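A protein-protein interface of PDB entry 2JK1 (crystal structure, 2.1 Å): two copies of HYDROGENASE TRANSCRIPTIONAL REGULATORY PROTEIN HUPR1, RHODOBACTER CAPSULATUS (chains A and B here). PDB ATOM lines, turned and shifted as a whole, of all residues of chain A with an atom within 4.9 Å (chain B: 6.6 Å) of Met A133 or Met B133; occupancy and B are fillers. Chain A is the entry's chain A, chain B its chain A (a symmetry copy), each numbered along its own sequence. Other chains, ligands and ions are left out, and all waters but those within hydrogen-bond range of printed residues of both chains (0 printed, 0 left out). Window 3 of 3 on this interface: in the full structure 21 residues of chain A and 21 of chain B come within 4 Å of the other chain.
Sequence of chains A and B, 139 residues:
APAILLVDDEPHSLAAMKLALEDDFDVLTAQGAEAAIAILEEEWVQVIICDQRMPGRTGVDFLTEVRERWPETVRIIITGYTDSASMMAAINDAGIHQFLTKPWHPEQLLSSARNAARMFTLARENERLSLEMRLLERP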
ATOM      1  N   LEU A 129      14.355   2.480 -19.463  1.00  0.00           N
ATOM      2  CA  LEU A 129      14.632   1.367 -20.353  1.00  0.00           C
ATOM      3  C   LEU A 129      15.404   0.262 -19.622  1.00  0.00           C
ATOM      4  O   LEU A 129      15.060  -0.919 -19.761  1.00  0.00           O
ATOM      5  CB  LEU A 129      15.337   1.812 -21.660  1.00  0.00           C
ATOM      6  CG  LEU A 129      14.487   2.548 -22.715  1.00  0.00           C
ATOM      7  CD1 LEU A 129      15.327   3.267 -23.808  1.00  0.00           C
ATOM      8  CD2 LEU A 129      13.453   1.594 -23.370  1.00  0.00           C
ATOM      9  N   SER A 130      16.412   0.627 -18.828  1.00  0.00           N
ATOM     10  CA  SER A 130      17.153  -0.391 -18.054  1.00  0.00           C
ATOM     11  C   SER A 130      16.254  -1.106 -17.046  1.00  0.00           C
ATOM     12  O   SER A 130      16.351  -2.329 -16.886  1.00  0.00           O
ATOM     13  CB  SER A 130      18.394   0.186 -17.365  1.00  0.00           C
ATOM     14  OG  SER A 130      18.030   1.211 -16.452  1.00  0.00           O
ATOM     15  N   LEU A 131      15.355  -0.362 -16.396  1.00  0.00           N
ATOM     16  CA  LEU A 131      14.393  -0.981 -15.473  1.00  0.00           C
ATOM     17  C   LEU A 131      13.396  -1.942 -16.166  1.00  0.00           C
ATOM     18  O   LEU A 131      13.173  -3.057 -15.675  1.00  0.00           O
ATOM     19  CB  LEU A 131      13.668   0.055 -14.607  1.00  0.00           C
ATOM     20  CG  LEU A 131      14.541   0.885 -13.651  1.00  0.00           C
ATOM     21  CD1 LEU A 131      13.718   1.989 -12.947  1.00  0.00           C
ATOM     22  CD2 LEU A 131      15.274   0.008 -12.662  1.00  0.00           C
ATOM     23  N   GLU A 132      12.813  -1.508 -17.282  1.00  0.00           N
ATOM     24  CA  GLU A 132      11.916  -2.350 -18.088  1.00  0.00           C
ATOM     25  C   GLU A 132      12.585  -3.633 -18.604  1.00  0.00           C
ATOM     26  O   GLU A 132      11.917  -4.659 -18.773  1.00  0.00           O
ATOM     27  CB  GLU A 132      11.309  -1.559 -19.255  1.00  0.00           C
ATOM     28  CG  GLU A 132      10.312  -0.463 -18.839  1.00  0.00           C
ATOM     29  CD  GLU A 132       8.895  -0.975 -18.542  1.00  0.00           C
ATOM     30  OE1 GLU A 132       8.637  -2.195 -18.606  1.00  0.00           O
ATOM     31  OE2 GLU A 132       8.021  -0.138 -18.243  1.00  0.00           O
ATOM     32  N   MET A 133      13.893  -3.570 -18.849  1.00  0.00           N
ATOM     33  CA  MET A 133      14.685  -4.751 -19.220  1.00  0.00           C
ATOM     34  C   MET A 133      14.754  -5.791 -18.082  1.00  0.00           C
ATOM     35  O   MET A 133      14.656  -6.995 -18.347  1.00  0.00           O
ATOM     36  CB  MET A 133      16.085  -4.337 -19.660  1.00  0.00           C
ATOM     37  CG  MET A 133      16.136  -3.784 -21.064  1.00  0.00           C
ATOM     38  SD  MET A 133      17.704  -4.054 -21.917  1.00  0.00           S
ATOM     39  CE  MET A 133      17.921  -5.810 -21.669  1.00  0.00           C
ATOM     40  N   ARG A 134      14.882  -5.320 -16.831  1.00  0.00           N
ATOM     41  CA  ARG A 134      14.789  -6.164 -15.632  1.00  0.00           C
ATOM     42  C   ARG A 134      13.421  -6.821 -15.465  1.00  0.00           C
ATOM     43  O   ARG A 134      13.316  -7.939 -14.949  1.00  0.00           O
ATOM     44  CB  ARG A 134      15.076  -5.349 -14.353  1.00  0.00           C
ATOM     45  CG  ARG A 134      14.748  -6.097 -13.029  1.00  0.00           C
ATOM     46  CD  ARG A 134      15.660  -7.308 -12.825  1.00  0.00           C
ATOM     47  NE  ARG A 134      15.575  -8.033 -11.536  1.00  0.00           N
ATOM     48  CZ  ARG A 134      14.688  -8.972 -11.259  1.00  0.00           C
ATOM     49  NH1 ARG A 134      13.749  -9.275 -12.151  1.00  0.00           N
ATOM     50  NH2 ARG A 134      14.760  -9.626 -10.115  1.00  0.00           N
ATOM     51  N   LEU A 135      12.366  -6.117 -15.843  1.00  0.00           N
ATOM     52  CA  LEU A 135      11.039  -6.698 -15.760  1.00  0.00           C
ATOM     53  C   LEU A 135      10.813  -7.731 -16.868  1.00  0.00           C
ATOM     54  O   LEU A 135       9.910  -8.574 -16.740  1.00  0.00           O
ATOM     55  CB  LEU A 135       9.953  -5.622 -15.713  1.00  0.00           C
ATOM     56  CG  LEU A 135      10.035  -4.699 -14.489  1.00  0.00           C
ATOM     57  CD1 LEU A 135       8.868  -3.750 -14.528  1.00  0.00           C
ATOM     58  CD2 LEU A 135      10.104  -5.495 -13.158  1.00  0.00           C
ATOM     59  N   LEU A 136      11.654  -7.689 -17.916  1.00  0.00           N
ATOM     60  CA  LEU A 136      11.688  -8.738 -18.973  1.00  0.00           C
ATOM     61  C   LEU A 136      12.735  -9.868 -18.787  1.00  0.00           C
ATOM     62  O   LEU A 136      12.461 -11.010 -19.126  1.00  0.00           O
ATOM     63  CB  LEU A 136      11.851  -8.130 -20.380  1.00  0.00           C
ATOM     64  CG  LEU A 136      10.815  -7.144 -20.935  1.00  0.00           C
ATOM     65  CD1 LEU A 136      11.250  -6.653 -22.327  1.00  0.00           C
ATOM     66  CD2 LEU A 136       9.404  -7.747 -20.975  1.00  0.00           C
ATOM     67  N   GLU A 137      13.926  -9.527 -18.297  1.00  0.00           N
ATOM     68  CA  GLU A 137      15.049 -10.455 -18.096  1.00  0.00           C
ATOM     69  C   GLU A 137      15.031 -11.064 -16.693  1.00  0.00           C
ATOM     70  O   GLU A 137      14.423 -10.518 -15.791  1.00  0.00           O
ATOM     71  CB  GLU A 137      16.367  -9.684 -18.212  1.00  0.00           C
ATOM     72  CG  GLU A 137      17.241  -9.925 -19.422  1.00  0.00           C
ATOM     73  CD  GLU A 137      18.330  -8.845 -19.571  1.00  0.00           C
ATOM     74  OE1 GLU A 137      18.511  -8.015 -18.649  1.00  0.00           O
ATOM     75  OE2 GLU A 137      19.016  -8.825 -20.614  1.00  0.00           O
ATOM     76  N   ARG B 128      20.676   1.590 -28.119  1.00  0.00           N
ATOM     77  CA  ARG B 128      21.107   0.239 -27.791  1.00  0.00           C
ATOM     78  C   ARG B 128      20.131  -0.490 -26.861  1.00  0.00           C
ATOM     79  O   ARG B 128      19.816  -1.657 -27.094  1.00  0.00           O
ATOM     80  CB  ARG B 128      22.510   0.266 -27.183  1.00  0.00           C
ATOM     81  CG  ARG B 128      23.078  -1.097 -26.757  1.00  0.00           C
ATOM     82  CD  ARG B 128      24.263  -0.890 -25.789  1.00  0.00           C
ATOM     83  NE  ARG B 128      23.835  -0.643 -24.402  1.00  0.00           N
ATOM     84  CZ  ARG B 128      23.467  -1.604 -23.548  1.00  0.00           C
ATOM     85  NH1 ARG B 128      23.475  -2.872 -23.918  1.00  0.00           N
ATOM     86  NH2 ARG B 128      23.097  -1.304 -22.312  1.00  0.00           N
ATOM     87  N   LEU B 129      19.666   0.194 -25.818  1.00  0.00           N
ATOM     88  CA  LEU B 129      18.726  -0.383 -24.874  1.00  0.00           C
ATOM     89  C   LEU B 129      17.392  -0.706 -25.560  1.00  0.00           C
ATOM     90  O   LEU B 129      16.845  -1.796 -25.349  1.00  0.00           O
ATOM     91  CB  LEU B 129      18.539   0.493 -23.609  1.00  0.00           C
ATOM     92  CG  LEU B 129      19.685   0.510 -22.578  1.00  0.00           C
ATOM     93  CD1 LEU B 129      19.582   1.667 -21.543  1.00  0.00           C
ATOM     94  CD2 LEU B 129      19.808  -0.855 -21.849  1.00  0.00           C
ATOM     95  N   SER B 130      16.885   0.203 -26.394  1.00  0.00           N
ATOM     96  CA  SER B 130      15.633  -0.080 -27.127  1.00  0.00           C
ATOM     97  C   SER B 130      15.784  -1.268 -28.075  1.00  0.00           C
ATOM     98  O   SER B 130      14.877  -2.105 -28.170  1.00  0.00           O
ATOM     99  CB  SER B 130      15.101   1.149 -27.873  1.00  0.00           C
ATOM    100  OG  SER B 130      16.045   1.601 -28.832  1.00  0.00           O
ATOM    101  N   LEU B 131      16.935  -1.371 -28.746  1.00  0.00           N
ATOM    102  CA  LEU B 131      17.199  -2.529 -29.612  1.00  0.00           C
ATOM    103  C   LEU B 131      17.291  -3.871 -28.847  1.00  0.00           C
ATOM    104  O   LEU B 131      16.685  -4.865 -29.271  1.00  0.00           O
ATOM    105  CB  LEU B 131      18.416  -2.311 -30.518  1.00  0.00           C
ATOM    106  CG  LEU B 131      18.321  -1.163 -31.536  1.00  0.00           C
ATOM    107  CD1 LEU B 131      19.659  -0.953 -32.282  1.00  0.00           C
ATOM    108  CD2 LEU B 131      17.166  -1.359 -32.492  1.00  0.00           C
ATOM    109  N   GLU B 132      18.037  -3.889 -27.744  1.00  0.00           N
ATOM    110  CA  GLU B 132      18.139  -5.072 -26.874  1.00  0.00           C
ATOM    111  C   GLU B 132      16.787  -5.527 -26.304  1.00  0.00           C
ATOM    112  O   GLU B 132      16.583  -6.721 -26.064  1.00  0.00           O
ATOM    113  CB  GLU B 132      19.147  -4.842 -25.740  1.00  0.00           C
ATOM    114  CG  GLU B 132      20.613  -4.742 -26.193  1.00  0.00           C
ATOM    115  CD  GLU B 132      21.298  -6.096 -26.431  1.00  0.00           C
ATOM    116  OE1 GLU B 132      20.658  -7.160 -26.295  1.00  0.00           O
ATOM    117  OE2 GLU B 132      22.501  -6.094 -26.757  1.00  0.00           O
ATOM    118  N   MET B 133      15.877  -4.578 -26.091  1.00  0.00           N
ATOM    119  CA  MET B 133      14.501  -4.881 -25.672  1.00  0.00           C
ATOM    120  C   MET B 133      13.719  -5.658 -26.754  1.00  0.00           C
ATOM    121  O   MET B 133      12.978  -6.590 -26.422  1.00  0.00           O
ATOM    122  CB  MET B 133      13.766  -3.603 -25.286  1.00  0.00           C
ATOM    123  CG  MET B 133      14.135  -3.088 -23.915  1.00  0.00           C
ATOM    124  SD  MET B 133      12.821  -2.172 -23.083  1.00  0.00           S
ATOM    125  CE  MET B 133      11.462  -3.322 -23.240  1.00  0.00           C
ATOM    126  N   ARG B 134      13.919  -5.295 -28.031  1.00  0.00           N
ATOM    127  CA  ARG B 134      13.387  -6.040 -29.180  1.00  0.00           C
ATOM    128  C   ARG B 134      13.940  -7.460 -29.281  1.00  0.00           C
ATOM    129  O   ARG B 134      13.245  -8.377 -29.733  1.00  0.00           O
ATOM    130  CB  ARG B 134      13.704  -5.319 -30.507  1.00  0.00           C
ATOM    131  CG  ARG B 134      13.407  -6.160 -31.781  1.00  0.00           C
ATOM    132  CD  ARG B 134      11.911  -6.436 -31.939  1.00  0.00           C
ATOM    133  NE  ARG B 134      11.453  -7.095 -33.184  1.00  0.00           N
ATOM    134  CZ  ARG B 134      11.458  -8.400 -33.390  1.00  0.00           C
ATOM    135  NH1 ARG B 134      11.959  -9.211 -32.463  1.00  0.00           N
ATOM    136  NH2 ARG B 134      10.936  -8.892 -34.498  1.00  0.00           N
ATOM    137  N   LEU B 135      15.199  -7.642 -28.919  1.00  0.00           N
ATOM    138  CA  LEU B 135      15.775  -8.974 -28.943  1.00  0.00           C
ATOM    139  C   LEU B 135      15.262  -9.822 -27.775  1.00  0.00           C
ATOM    140  O   LEU B 135      15.347 -11.059 -27.838  1.00  0.00           O
ATOM    141  CB  LEU B 135      17.302  -8.928 -29.025  1.00  0.00           C
ATOM    142  CG  LEU B 135      17.843  -8.264 -30.299  1.00  0.00           C
ATOM    143  CD1 LEU B 135      19.344  -8.362 -30.287  1.00  0.00           C
ATOM    144  CD2 LEU B 135      17.222  -8.872 -31.586  1.00  0.00           C
ATOM    145  N   LEU B 136      14.696  -9.162 -26.750  1.00  0.00           N
ATOM    146  CA  LEU B 136      13.981  -9.848 -25.638  1.00  0.00           C
ATOM    147  C   LEU B 136      12.441  -9.973 -25.784  1.00  0.00           C
ATOM    148  O   LEU B 136      11.873 -10.976 -25.378  1.00  0.00           O
ATOM    149  CB  LEU B 136      14.305  -9.216 -24.270  1.00  0.00           C
ATOM    150  CG  LEU B 136      15.746  -9.170 -23.748  1.00  0.00           C
ATOM    151  CD1 LEU B 136      15.792  -8.439 -22.394  1.00  0.00           C
ATOM    152  CD2 LEU B 136      16.371 -10.568 -23.645  1.00  0.00           C
ATOM    153  N   GLU B 137      11.789  -8.940 -26.317  1.00  0.00           N
ATOM    154  CA  GLU B 137      10.331  -8.865 -26.492  1.00  0.00           C
ATOM    155  C   GLU B 137       9.901  -9.400 -27.859  1.00  0.00           C
ATOM    156  O   GLU B 137      10.698  -9.464 -28.776  1.00  0.00           O
ATOM    157  CB  GLU B 137       9.893  -7.400 -26.446  1.00  0.00           C
ATOM    158  CG  GLU B 137       9.113  -6.916 -25.244  1.00  0.00           C
ATOM    159  CD  GLU B 137       9.054  -5.377 -25.177  1.00  0.00           C
ATOM    160  OE1 GLU B 137       9.465  -4.697 -26.147  1.00  0.00           O
ATOM    161  OE2 GLU B 137       8.586  -4.839 -24.152  1.00  0.00           O
ATOM    162  N   ARG B 138       8.626  -9.770 -27.975  1.00  0.00           N
ATOM    163  CA  ARG B 138       7.932 -10.014 -29.265  1.00  0.00           C
ATOM    164  C   ARG B 138       7.864 -11.452 -29.869  1.00  0.00           C
ATOM    165  O   ARG B 138       6.789 -11.834 -30.348  1.00  0.00           O
ATOM    166  CB  ARG B 138       8.266  -8.949 -30.333  1.00  0.00           C
ATOM    167  CG  ARG B 138       7.297  -7.768 -30.334  1.00  0.00           C
ATOM    168  CD  ARG B 138       7.598  -6.759 -31.445  1.00  0.00           C
ATOM    169  NE  ARG B 138       8.698  -5.805 -31.180  1.00  0.00           N
ATOM    170  CZ  ARG B 138       9.121  -5.350 -29.990  1.00  0.00           C
ATOM    171  NH1 ARG B 138       8.563  -5.728 -28.851  1.00  0.00           N
ATOM    172  NH2 ARG B 138      10.119  -4.474 -29.940  1.00  0.00           N
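The side-chain carboxylate (OE1) of Glu B137 lies within salt-bridge range of the guanidinium group (NH1) of Arg B138, 3.0 Å away.
Among the printed residues, merely in contact across the chains: Met A133 with Leu B136, Leu A136 with Met B133, Met A133 with Met B133, Glu A137 with Leu B136, Leu A136 with Glu B137, Leu A129 with Met B133, Met A133 with Leu B129 and Leu A129 with Leu B129.
Printed residues of chain B within 4 Å of Leu A129: Leu B129 (3.97 Å) and Met B133 (3.8 Å). Leu A131 touches none of the printed residues of chain B. Of the printed residues of chain B, Met A133 touches Leu B129 (3.8 Å), Met B133 (3.6 Å) and Leu B136 (3.5 Å). Printed residues of chain B within 4 Å of Glu A137: Leu B136 (3.6 Å). Printed residues of chain A within 4 Å of Leu B129: Leu A129 (3.97 Å) and Met A133 (3.8 Å). Printed residues of chain A within 4 Å of Met B133: Leu A129, Met A133 and Leu A136. Arg B134 touches none of the printed residues of chain A. Printed residues of chain A within 4 Å of Leu B136: Met A133 (3.5 Å) and Glu A137 (3.6 Å). Of the printed residues of chain A, Glu B137 touches Leu A136. The nearest printed residue of chain A that does not touch Met B133 is Glu A132 (4.2 Å). The nearest printed residue of chain B that does not touch Leu A136 is Leu B136 (4.4 Å).
Hydrophobic or aromatic side chains of chain A within 4 Å of the printed part of chain B: Leu A129, Met A133 and Leu A136. Hydrophobic or aromatic side chains of chain B that line the printed part of chain A: Leu B129, Met B133 and Leu B136. Among the printed residues, no Asp or Glu carboxylate lies within 4 Å of a Lys or Arg side-chain nitrogen of the other chain.
Leu A129 touches its own counterpart, Leu B129. Met B133 touches its own counterpart, Met A133. Met A133 touches Leu B136, and with the chains exchanged Leu A136 touches Met B133. Leu A136 touches Glu B137, and with the chains exchanged Glu A137 touches Leu B136. Positions printed for both chains: 129, 130, 131, 132, 133, 134, 135, 136 and 137.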
